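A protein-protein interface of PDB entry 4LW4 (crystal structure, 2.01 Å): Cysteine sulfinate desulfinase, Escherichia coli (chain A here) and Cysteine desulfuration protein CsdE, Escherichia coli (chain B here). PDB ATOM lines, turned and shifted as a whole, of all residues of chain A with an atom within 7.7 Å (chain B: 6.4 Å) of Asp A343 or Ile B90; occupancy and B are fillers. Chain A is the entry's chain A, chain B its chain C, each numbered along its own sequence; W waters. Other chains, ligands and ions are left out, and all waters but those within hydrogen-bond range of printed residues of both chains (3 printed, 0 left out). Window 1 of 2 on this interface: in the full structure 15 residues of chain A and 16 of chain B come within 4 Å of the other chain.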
ATOM      1  N   GLY A 338     -30.643 -29.955 -29.263  1.00  0.00           N
ATOM      2  CA  GLY A 338     -31.161 -28.738 -28.644  1.00  0.00           C
ATOM      3  C   GLY A 338     -30.213 -28.081 -27.618  1.00  0.00           C
ATOM      4  O   GLY A 338     -30.639 -27.247 -26.839  1.00  0.00           O
ATOM      5  N   VAL A 339     -28.950 -28.461 -27.588  1.00  0.00           N
ATOM      6  CA  VAL A 339     -28.004 -27.843 -26.644  1.00  0.00           C
ATOM      7  C   VAL A 339     -26.861 -27.330 -27.512  1.00  0.00           C
ATOM      8  O   VAL A 339     -26.300 -28.100 -28.338  1.00  0.00           O
ATOM      9  CB  VAL A 339     -27.432 -28.899 -25.673  1.00  0.00           C
ATOM     10  CG1 VAL A 339     -26.240 -28.327 -24.816  1.00  0.00           C
ATOM     11  CG2 VAL A 339     -28.551 -29.461 -24.784  1.00  0.00           C
ATOM     12  N   HIS A 340     -26.480 -26.070 -27.332  1.00  0.00           N
ATOM     13  CA  HIS A 340     -25.374 -25.577 -28.151  1.00  0.00           C
ATOM     14  C   HIS A 340     -24.057 -25.978 -27.467  1.00  0.00           C
ATOM     15  O   HIS A 340     -23.934 -25.886 -26.245  1.00  0.00           O
ATOM     16  CB  HIS A 340     -25.492 -24.062 -28.381  1.00  0.00           C
ATOM     17  CG  HIS A 340     -24.422 -23.504 -29.277  1.00  0.00           C
ATOM     18  ND1 HIS A 340     -24.614 -23.286 -30.631  1.00  0.00           N
ATOM     19  CD2 HIS A 340     -23.146 -23.155 -29.022  1.00  0.00           C
ATOM     20  CE1 HIS A 340     -23.503 -22.802 -31.160  1.00  0.00           C
ATOM     21  NE2 HIS A 340     -22.602 -22.709 -30.205  1.00  0.00           N
ATOM     22  N   HIS A 341     -23.104 -26.461 -28.261  1.00  0.00           N
ATOM     23  CA  HIS A 341     -21.818 -26.889 -27.752  1.00  0.00           C
ATOM     24  C   HIS A 341     -21.069 -25.859 -26.892  1.00  0.00           C
ATOM     25  O   HIS A 341     -20.371 -26.257 -25.932  1.00  0.00           O
ATOM     26  CB  HIS A 341     -20.887 -27.429 -28.891  1.00  0.00           C
ATOM     27  CG  HIS A 341     -20.900 -26.571 -30.116  1.00  0.00           C
ATOM     28  ND1 HIS A 341     -20.021 -25.518 -30.301  1.00  0.00           N
ATOM     29  CD2 HIS A 341     -21.749 -26.547 -31.170  1.00  0.00           C
ATOM     30  CE1 HIS A 341     -20.302 -24.918 -31.446  1.00  0.00           C
ATOM     31  NE2 HIS A 341     -21.338 -25.528 -31.993  1.00  0.00           N
ATOM     32  N   SER A 342     -21.219 -24.573 -27.216  1.00  0.00           N
ATOM     33  CA  SER A 342     -20.641 -23.472 -26.432  1.00  0.00           C
ATOM     34  C   SER A 342     -21.137 -23.455 -24.996  1.00  0.00           C
ATOM     35  O   SER A 342     -20.375 -23.180 -24.040  1.00  0.00           O
ATOM     36  CB  SER A 342     -21.147 -22.117 -26.995  1.00  0.00           C
ATOM     37  OG  SER A 342     -20.139 -21.596 -27.797  1.00  0.00           O
ATOM     38  N   ASP A 343     -22.438 -23.646 -24.852  1.00  0.00           N
ATOM     39  CA  ASP A 343     -23.044 -23.557 -23.532  1.00  0.00           C
ATOM     40  C   ASP A 343     -22.529 -24.765 -22.730  1.00  0.00           C
ATOM     41  O   ASP A 343     -22.124 -24.611 -21.628  1.00  0.00           O
ATOM     42  CB  ASP A 343     -24.575 -23.553 -23.607  1.00  0.00           C
ATOM     43  CG  ASP A 343     -25.143 -22.302 -24.271  1.00  0.00           C
ATOM     44  OD1 ASP A 343     -24.580 -21.194 -24.070  1.00  0.00           O
ATOM     45  OD2 ASP A 343     -26.127 -22.435 -25.060  1.00  0.00           O
ATOM     46  N   MET A 344     -22.528 -25.943 -23.325  1.00  0.00           N
ATOM     47  CA  MET A 344     -22.066 -27.122 -22.615  1.00  0.00           C
ATOM     48  C   MET A 344     -20.565 -26.990 -22.197  1.00  0.00           C
ATOM     49  O   MET A 344     -20.198 -27.303 -21.039  1.00  0.00           O
ATOM     50  CB  MET A 344     -22.307 -28.397 -23.419  1.00  0.00           C
ATOM     51  CG  MET A 344     -21.919 -29.629 -22.504  1.00  0.00           C
ATOM     52  SD  MET A 344     -23.149 -30.941 -22.531  1.00  0.00           S
ATOM     53  CE  MET A 344     -24.496 -29.906 -22.034  1.00  0.00           C
ATOM     54  N   VAL A 345     -19.713 -26.509 -23.105  1.00  0.00           N
ATOM     55  CA  VAL A 345     -18.256 -26.430 -22.803  1.00  0.00           C
ATOM     56  C   VAL A 345     -18.007 -25.475 -21.648  1.00  0.00           C
ATOM     57  O   VAL A 345     -17.175 -25.731 -20.756  1.00  0.00           O
ATOM     58  CB  VAL A 345     -17.385 -26.098 -24.068  1.00  0.00           C
ATOM     59  CG1 VAL A 345     -17.579 -24.637 -24.518  1.00  0.00           C
ATOM     60  CG2 VAL A 345     -15.863 -26.282 -23.772  1.00  0.00           C
ATOM     61  N   THR A 346     -18.762 -24.379 -21.637  1.00  0.00           N
ATOM     62  CA  THR A 346     -18.693 -23.398 -20.549  1.00  0.00           C
ATOM     63  C   THR A 346     -19.094 -24.020 -19.213  1.00  0.00           C
ATOM     64  O   THR A 346     -18.350 -23.911 -18.228  1.00  0.00           O
ATOM     65  CB  THR A 346     -19.607 -22.181 -20.838  1.00  0.00           C
ATOM     66  OG1 THR A 346     -19.023 -21.492 -21.946  1.00  0.00           O
ATOM     67  CG2 THR A 346     -19.629 -21.211 -19.678  1.00  0.00           C
ATOM     68  N   LEU A 347     -20.274 -24.643 -19.170  1.00  0.00           N
ATOM     69  CA  LEU A 347     -20.712 -25.246 -17.884  1.00  0.00           C
ATOM     70  C   LEU A 347     -19.739 -26.333 -17.435  1.00  0.00           C
ATOM     71  O   LEU A 347     -19.409 -26.415 -16.244  1.00  0.00           O
ATOM     72  CB  LEU A 347     -22.115 -25.801 -17.982  1.00  0.00           C
ATOM     73  CG  LEU A 347     -23.143 -24.689 -18.195  1.00  0.00           C
ATOM     74  CD1 LEU A 347     -24.496 -25.309 -18.237  1.00  0.00           C
ATOM     75  CD2 LEU A 347     -23.102 -23.614 -17.079  1.00  0.00           C
ATOM     76  N   LEU A 348     -19.256 -27.132 -18.385  1.00  0.00           N
ATOM     77  CA  LEU A 348     -18.379 -28.238 -18.008  1.00  0.00           C
ATOM     78  C   LEU A 348     -17.125 -27.672 -17.347  1.00  0.00           C
ATOM     79  O   LEU A 348     -16.668 -28.251 -16.375  1.00  0.00           O
ATOM     80  CB  LEU A 348     -18.004 -29.154 -19.199  1.00  0.00           C
ATOM     81  CG  LEU A 348     -18.835 -30.466 -19.401  1.00  0.00           C
ATOM     82  CD1 LEU A 348     -20.289 -30.336 -19.038  1.00  0.00           C
ATOM     83  CD2 LEU A 348     -18.683 -31.048 -20.866  1.00  0.00           C
ATOM     84  N   ALA A 349     -16.568 -26.581 -17.910  1.00  0.00           N
ATOM     85  CA  ALA A 349     -15.385 -25.936 -17.340  1.00  0.00           C
ATOM     86  C   ALA A 349     -15.655 -25.429 -15.906  1.00  0.00           C
ATOM     87  O   ALA A 349     -14.805 -25.642 -15.031  1.00  0.00           O
ATOM     88  CB  ALA A 349     -14.854 -24.799 -18.248  1.00  0.00           C
ATOM     89  N   GLU A 350     -16.830 -24.803 -15.686  1.00  0.00           N
ATOM     90  CA  GLU A 350     -17.258 -24.415 -14.355  1.00  0.00           C
ATOM     91  C   GLU A 350     -17.347 -25.653 -13.417  1.00  0.00           C
ATOM     92  O   GLU A 350     -17.001 -25.553 -12.242  1.00  0.00           O
ATOM     93  CB  GLU A 350     -18.647 -23.742 -14.405  1.00  0.00           C
ATOM     94  CG  GLU A 350     -18.647 -22.444 -15.269  1.00  0.00           C
ATOM     95  CD  GLU A 350     -18.129 -21.212 -14.511  1.00  0.00           C
ATOM     96  OE1 GLU A 350     -17.298 -21.337 -13.574  1.00  0.00           O
ATOM     97  OE2 GLU A 350     -18.549 -20.086 -14.843  1.00  0.00           O
ATOM     98  N   ALA A 357     -14.856 -27.234 -27.708  1.00  0.00           N
ATOM     99  CA  ALA A 357     -16.034 -27.175 -28.569  1.00  0.00           C
ATOM    100  C   ALA A 357     -15.669 -26.381 -29.842  1.00  0.00           C
ATOM    101  O   ALA A 357     -14.674 -25.693 -29.854  1.00  0.00           O
ATOM    102  CB  ALA A 357     -17.151 -26.518 -27.843  1.00  0.00           C
ATOM    103  N   LEU A 375     -18.863 -30.892 -29.427  1.00  0.00           N
ATOM    104  CA  LEU A 375     -17.978 -30.976 -28.281  1.00  0.00           C
ATOM    105  C   LEU A 375     -17.006 -32.093 -28.570  1.00  0.00           C
ATOM    106  O   LEU A 375     -17.349 -32.996 -29.394  1.00  0.00           O
ATOM    107  CB  LEU A 375     -18.780 -31.359 -27.041  1.00  0.00           C
ATOM    108  CG  LEU A 375     -19.800 -30.380 -26.525  1.00  0.00           C
ATOM    109  CD1 LEU A 375     -21.209 -30.820 -26.780  1.00  0.00           C
ATOM    110  CD2 LEU A 375     -19.625 -30.376 -25.044  1.00  0.00           C
ATOM    111  N   ALA A 398     -24.976 -30.128 -16.254  1.00  0.00           N
ATOM    112  CA  ALA A 398     -25.132 -29.136 -17.324  1.00  0.00           C
ATOM    113  C   ALA A 398     -26.477 -29.305 -18.037  1.00  0.00           C
ATOM    114  O   ALA A 398     -27.143 -28.326 -18.265  1.00  0.00           O
ATOM    115  CB  ALA A 398     -23.981 -29.295 -18.373  1.00  0.00           C
ATOM    116  N   LEU A 401     -29.403 -27.692 -16.408  1.00  0.00           N
ATOM    117  CA  LEU A 401     -29.423 -26.263 -16.581  1.00  0.00           C
ATOM    118  C   LEU A 401     -29.869 -25.878 -18.014  1.00  0.00           C
ATOM    119  O   LEU A 401     -30.506 -24.854 -18.195  1.00  0.00           O
ATOM    120  CB  LEU A 401     -28.012 -25.683 -16.301  1.00  0.00           C
ATOM    121  CG  LEU A 401     -27.833 -24.482 -15.369  1.00  0.00           C
ATOM    122  CD1 LEU A 401     -26.397 -24.325 -14.819  1.00  0.00           C
ATOM    123  CD2 LEU A 401     -28.249 -23.191 -16.186  1.00  0.00           C
ATOM    124  N   LEU A 402     -29.483 -26.653 -19.032  1.00  0.00           N
ATOM    125  CA  LEU A 402     -29.734 -26.272 -20.452  1.00  0.00           C
ATOM    126  C   LEU A 402     -31.018 -26.797 -21.201  1.00  0.00           C
ATOM    127  O   LEU A 402     -31.330 -26.312 -22.306  1.00  0.00           O
ATOM    128  CB  LEU A 402     -28.513 -26.656 -21.296  1.00  0.00           C
ATOM    129  CG  LEU A 402     -27.198 -26.030 -20.864  1.00  0.00           C
ATOM    130  CD1 LEU A 402     -25.992 -26.630 -21.568  1.00  0.00           C
ATOM    131  CD2 LEU A 402     -27.273 -24.524 -21.134  1.00  0.00           C
ATOM    132  N   TYR B  37     -26.398 -18.393 -14.383  1.00  0.00           N
ATOM    133  CA  TYR B  37     -26.426 -18.915 -15.759  1.00  0.00           C
ATOM    134  C   TYR B  37     -27.880 -19.216 -16.192  1.00  0.00           C
ATOM    135  O   TYR B  37     -28.288 -18.847 -17.279  1.00  0.00           O
ATOM    136  CB  TYR B  37     -25.542 -20.167 -15.925  1.00  0.00           C
ATOM    137  CG  TYR B  37     -24.061 -19.879 -16.110  1.00  0.00           C
ATOM    138  CD1 TYR B  37     -23.606 -19.032 -17.138  1.00  0.00           C
ATOM    139  CD2 TYR B  37     -23.109 -20.462 -15.262  1.00  0.00           C
ATOM    140  CE1 TYR B  37     -22.215 -18.763 -17.325  1.00  0.00           C
ATOM    141  CE2 TYR B  37     -21.747 -20.171 -15.380  1.00  0.00           C
ATOM    142  CZ  TYR B  37     -21.299 -19.356 -16.422  1.00  0.00           C
ATOM    143  OH  TYR B  37     -19.985 -19.062 -16.534  1.00  0.00           O
ATOM    144  N   LEU B  40     -29.467 -15.927 -17.067  1.00  0.00           N
ATOM    145  CA  LEU B  40     -28.871 -15.416 -18.353  1.00  0.00           C
ATOM    146  C   LEU B  40     -29.537 -16.111 -19.561  1.00  0.00           C
ATOM    147  O   LEU B  40     -29.947 -15.491 -20.560  1.00  0.00           O
ATOM    148  CB  LEU B  40     -27.319 -15.571 -18.356  1.00  0.00           C
ATOM    149  CG  LEU B  40     -26.592 -14.509 -17.489  1.00  0.00           C
ATOM    150  CD1 LEU B  40     -25.100 -14.967 -17.175  1.00  0.00           C
ATOM    151  CD2 LEU B  40     -26.621 -13.088 -18.194  1.00  0.00           C
ATOM    152  N   ILE B  41     -29.653 -17.409 -19.454  1.00  0.00           N
ATOM    153  CA  ILE B  41     -30.296 -18.192 -20.504  1.00  0.00           C
ATOM    154  C   ILE B  41     -31.729 -17.707 -20.748  1.00  0.00           C
ATOM    155  O   ILE B  41     -32.114 -17.432 -21.905  1.00  0.00           O
ATOM    156  CB  ILE B  41     -30.221 -19.673 -20.183  1.00  0.00           C
ATOM    157  CG1 ILE B  41     -28.756 -20.118 -20.274  1.00  0.00           C
ATOM    158  CG2 ILE B  41     -31.116 -20.472 -21.167  1.00  0.00           C
ATOM    159  CD1 ILE B  41     -28.410 -21.474 -19.674  1.00  0.00           C
ATOM    160  N   GLU B  65     -15.452 -21.415 -30.320  1.00  0.00           N
ATOM    161  CA  GLU B  65     -16.659 -22.106 -29.909  1.00  0.00           C
ATOM    162  C   GLU B  65     -18.022 -21.545 -30.378  1.00  0.00           C
ATOM    163  O   GLU B  65     -18.960 -22.324 -30.549  1.00  0.00           O
ATOM    164  CB  GLU B  65     -16.689 -22.154 -28.376  1.00  0.00           C
ATOM    165  CG  GLU B  65     -15.350 -22.370 -27.689  1.00  0.00           C
ATOM    166  CD  GLU B  65     -15.500 -22.386 -26.175  1.00  0.00           C
ATOM    167  OE1 GLU B  65     -14.530 -22.749 -25.476  1.00  0.00           O
ATOM    168  OE2 GLU B  65     -16.610 -22.052 -25.683  1.00  0.00           O
ATOM    169  N   SER B  86     -26.276 -14.301 -30.965  1.00  0.00           N
ATOM    170  CA  SER B  86     -25.243 -15.260 -30.518  1.00  0.00           C
ATOM    171  C   SER B  86     -25.819 -16.600 -30.759  1.00  0.00           C
ATOM    172  O   SER B  86     -26.968 -16.776 -30.530  1.00  0.00           O
ATOM    173  CB  SER B  86     -24.956 -15.106 -28.992  1.00  0.00           C
ATOM    174  OG  SER B  86     -24.188 -16.211 -28.470  1.00  0.00           O
ATOM    175  N   GLU B  87     -25.045 -17.594 -31.145  1.00  0.00           N
ATOM    176  CA  GLU B  87     -25.646 -18.932 -31.204  1.00  0.00           C
ATOM    177  C   GLU B  87     -25.835 -19.566 -29.813  1.00  0.00           C
ATOM    178  O   GLU B  87     -26.887 -20.139 -29.496  1.00  0.00           O
ATOM    179  CB  GLU B  87     -24.773 -19.864 -32.026  1.00  0.00           C
ATOM    180  CG  GLU B  87     -24.354 -19.334 -33.374  1.00  0.00           C
ATOM    181  CD  GLU B  87     -23.439 -20.327 -34.098  1.00  0.00           C
ATOM    182  OE1 GLU B  87     -22.286 -20.574 -33.622  1.00  0.00           O
ATOM    183  OE2 GLU B  87     -23.930 -20.894 -35.104  1.00  0.00           O
ATOM    184  N   GLY B  88     -24.815 -19.448 -28.966  1.00  0.00           N
ATOM    185  CA  GLY B  88     -24.866 -20.084 -27.598  1.00  0.00           C
ATOM    186  C   GLY B  88     -25.855 -19.280 -26.782  1.00  0.00           C
ATOM    187  O   GLY B  88     -25.877 -18.039 -26.898  1.00  0.00           O
ATOM    188  N   ARG B  89     -26.624 -19.948 -25.911  1.00  0.00           N
ATOM    189  CA  ARG B  89     -27.678 -19.284 -25.129  1.00  0.00           C
ATOM    190  C   ARG B  89     -27.139 -18.515 -23.957  1.00  0.00           C
ATOM    191  O   ARG B  89     -27.757 -17.514 -23.544  1.00  0.00           O
ATOM    192  CB  ARG B  89     -28.676 -20.293 -24.624  1.00  0.00           C
ATOM    193  CG  ARG B  89     -29.314 -21.108 -25.873  1.00  0.00           C
ATOM    194  CD  ARG B  89     -30.324 -22.186 -25.460  1.00  0.00           C
ATOM    195  NE  ARG B  89     -31.508 -21.530 -24.896  1.00  0.00           N
ATOM    196  CZ  ARG B  89     -32.349 -22.089 -24.016  1.00  0.00           C
ATOM    197  NH1 ARG B  89     -32.145 -23.341 -23.598  1.00  0.00           N
ATOM    198  NH2 ARG B  89     -33.382 -21.381 -23.548  1.00  0.00           N
ATOM    199  N   ILE B  90     -26.018 -18.995 -23.406  1.00  0.00           N
ATOM    200  CA  ILE B  90     -25.383 -18.266 -22.306  1.00  0.00           C
ATOM    201  C   ILE B  90     -24.856 -16.910 -22.793  1.00  0.00           C
ATOM    202  O   ILE B  90     -25.133 -15.840 -22.190  1.00  0.00           O
ATOM    203  CB  ILE B  90     -24.247 -19.091 -21.676  1.00  0.00           C
ATOM    204  CG1 ILE B  90     -24.838 -20.222 -20.779  1.00  0.00           C
ATOM    205  CG2 ILE B  90     -23.321 -18.187 -20.818  1.00  0.00           C
ATOM    206  CD1 ILE B  90     -23.836 -21.345 -20.304  1.00  0.00           C
ATOM    207  N   VAL B  91     -24.099 -16.947 -23.879  1.00  0.00           N
ATOM    208  CA  VAL B  91     -23.527 -15.702 -24.429  1.00  0.00           C
ATOM    209  C   VAL B  91     -24.648 -14.735 -24.951  1.00  0.00           C
ATOM    210  O   VAL B  91     -24.484 -13.486 -24.857  1.00  0.00           O
ATOM    211  CB  VAL B  91     -22.371 -15.973 -25.471  1.00  0.00           C
ATOM    212  CG1 VAL B  91     -21.971 -14.632 -26.177  1.00  0.00           C
ATOM    213  CG2 VAL B  91     -21.115 -16.651 -24.755  1.00  0.00           C
ATOM    214  N   ARG B  92     -25.775 -15.295 -25.445  1.00  0.00           N
ATOM    215  CA  ARG B  92     -26.973 -14.496 -25.808  1.00  0.00           C
ATOM    216  C   ARG B  92     -27.496 -13.708 -24.600  1.00  0.00           C
ATOM    217  O   ARG B  92     -27.886 -12.531 -24.722  1.00  0.00           O
ATOM    218  CB  ARG B  92     -28.083 -15.409 -26.409  1.00  0.00           C
ATOM    219  CG  ARG B  92     -29.424 -14.728 -26.782  1.00  0.00           C
ATOM    220  CD  ARG B  92     -30.395 -15.776 -27.494  1.00  0.00           C
ATOM    221  NE  ARG B  92     -29.596 -16.783 -28.220  1.00  0.00           N
ATOM    222  CZ  ARG B  92     -30.039 -17.925 -28.753  1.00  0.00           C
ATOM    223  NH1 ARG B  92     -31.324 -18.280 -28.715  1.00  0.00           N
ATOM    224  NH2 ARG B  92     -29.172 -18.730 -29.348  1.00  0.00           N
ATOM    225  N   GLY B  93     -27.499 -14.336 -23.424  1.00  0.00           N
ATOM    226  CA  GLY B  93     -27.920 -13.643 -22.175  1.00  0.00           C
ATOM    227  C   GLY B  93     -26.891 -12.538 -21.836  1.00  0.00           C
ATOM    228  O   GLY B  93     -27.264 -11.403 -21.414  1.00  0.00           O
ATOM    229  N   LEU B  94     -25.597 -12.859 -21.973  1.00  0.00           N
ATOM    230  CA  LEU B  94     -24.554 -11.832 -21.690  1.00  0.00           C
ATOM    231  C   LEU B  94     -24.699 -10.669 -22.680  1.00  0.00           C
ATOM    232  O   LEU B  94     -24.606  -9.495 -22.320  1.00  0.00           O
ATOM    233  CB  LEU B  94     -23.135 -12.405 -21.691  1.00  0.00           C
ATOM    234  CG  LEU B  94     -22.977 -13.457 -20.581  1.00  0.00           C
ATOM    235  CD1 LEU B  94     -21.795 -14.288 -21.001  1.00  0.00           C
ATOM    236  CD2 LEU B  94     -22.811 -12.798 -19.175  1.00  0.00           C
ATOM    237  N   LEU B  95     -24.984 -11.015 -23.923  1.00  0.00           N
ATOM    238  CA  LEU B  95     -25.228  -9.983 -24.932  1.00  0.00           C
ATOM    239  C   LEU B  95     -26.414  -9.085 -24.537  1.00  0.00           C
ATOM    240  O   LEU B  95     -26.346  -7.825 -24.622  1.00  0.00           O
ATOM    241  CB  LEU B  95     -25.377 -10.640 -26.340  1.00  0.00           C
ATOM    242  CG  LEU B  95     -25.715  -9.659 -27.484  1.00  0.00           C
ATOM    243  CD1 LEU B  95     -24.665  -8.525 -27.510  1.00  0.00           C
ATOM    244  CD2 LEU B  95     -25.771 -10.409 -28.799  1.00  0.00           C
ATOM    245  N   ALA B 130     -17.771 -17.258 -18.058  1.00  0.00           N
ATOM    246  CA  ALA B 130     -18.299 -16.819 -19.369  1.00  0.00           C
ATOM    247  C   ALA B 130     -18.214 -15.308 -19.467  1.00  0.00           C
ATOM    248  O   ALA B 130     -17.936 -14.788 -20.542  1.00  0.00           O
ATOM    249  CB  ALA B 130     -19.739 -17.228 -19.516  1.00  0.00           C
HETATM  250  O   HOH W   1     -22.893 -19.652 -24.898  1.00  0.00           O
HETATM  251  O   HOH W   2     -30.084 -25.415 -24.398  1.00  0.00           O
HETATM  252  O   HOH W   3     -13.706 -24.935 -26.889  1.00  0.00           O
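Among the printed residues, merely in contact across the chains: Val A345 with Glu B65 (3.0 Å), His A340 with Glu B87 (3.3 Å), Asp A343 with Gly B88 (3.6 Å), Leu A402 with Ile B41 (3.6 Å), Leu A347 with Tyr B37 (3.6 Å), His A340 with Glu B65 (3.7 Å), His A340 with Gly B88 (3.8 Å), Thr A346 with Tyr B37 (3.8 Å), Leu A401 with Ile B41 (3.9 Å), Thr A346 with Ala B130 (3.99 Å) and Leu A401 with Tyr B37 (3.99 Å).
O of Ser A342 lies within hydrogen-bond range of OG1 of Thr A346. The backbone NH (N) of Ala B130 sits at hydrogen-bond distance from the side-chain hydroxyl (OH) of Tyr B37. The backbone carbonyl oxygen (O) of Gly B88 sits at hydrogen-bond distance from the side-chain hydroxyl (OG) of Ser B86 (2.9 Å). The backbone carbonyl oxygen of Glu B87 is in hydrogen-bond range of the guanidinium group of Arg B92, 2.7 Å away.
Water W1 lies within hydrogen-bond range of the side-chain carboxylate (OD1) of Asp A343 (2.4 Å) and the backbone NH (N) of Val B91 (3.1 Å). Water W2 lies within hydrogen-bond range of the backbone carbonyl oxygen of Leu A402 (2.6 Å), the guanidinium group of Arg B89 (3.0 Å) and the backbone carbonyl oxygen of Gly A338 (3.1 Å). Water W3 bridges N of Ala A357 (2.7 Å) and OE1 of Glu B65 (2.7 Å).
Of the 15 printed residues of chain B, 8 touch a printed residue of chain A. Of the 18 printed residues of chain A, 10 touch a printed residue of chain B. Printed residues of chain A that touch a printed residue of chain B: His A340, His A341, Ser A342, Asp A343, Val A345, Thr A346, Leu A347, Glu A350, Leu A401 and Leu A402. Hydrophobic or aromatic side chains of chain A within 4 Å of the printed part of chain B: His A340, His A341, Val A345, Leu A347, Leu A401 and Leu A402. Among the printed residues, 17 pairs touch across the chains. Among the printed residues, no Asp or Glu carboxylate lies within 4 Å of a Lys or Arg side-chain nitrogen of the other chain.
O of Glu B65 lies close to ND1 of His A341 (3.4 Å). The side-chain hydroxyl of Ser A342 lies within hydrogen-bond range of the backbone carbonyl oxygen of Glu B65. The side-chain carboxylate (OD2) of Asp A343 lies within hydrogen-bond range of the backbone NH (N) of Arg B89 (2.7 Å). N of Ile B90 lies within hydrogen-bond range of OD1 of Asp A343. The side-chain hydroxyl of Tyr B37 lies within hydrogen-bond range of the side-chain carboxylate of Glu A350 (2.4 Å). The guanidinium group (NH1) of Arg B89 sits at hydrogen-bond distance from the backbone carbonyl oxygen (O) of Leu A402 (3.3 Å).
Asp A343 touches three residues of chain B. Met A344 touches none of the printed residues of chain B. Of the printed residues of chain B, Thr A346 touches Tyr B37 and Ala B130. Of the printed residues of chain B, Leu A402 touches Ile B41 and Arg B89. Of the printed residues of chain A, Tyr B37 touches Thr A346, Leu A347, Glu A350 and Leu A401. Printed residues of chain A within 4 Å of Glu B87: His A340 (3.3 Å). Printed residues of chain A within 4 Å of Gly B88: His A340 (3.8 Å) and Asp A343 (3.6 Å). Of the printed residues of chain A, Ile B90 touches Asp A343. Leu B95 touches none of the printed residues of chain A. The nearest residue of chain B that does not touch Asp A343 is Val B91 (4.3 Å). The nearest printed residue of chain A that does not touch Ile B90 is Leu A347 (4.01 Å). The nearest printed residue of chain A that does not touch Glu B65 is Ala A357 (4.02 Å).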
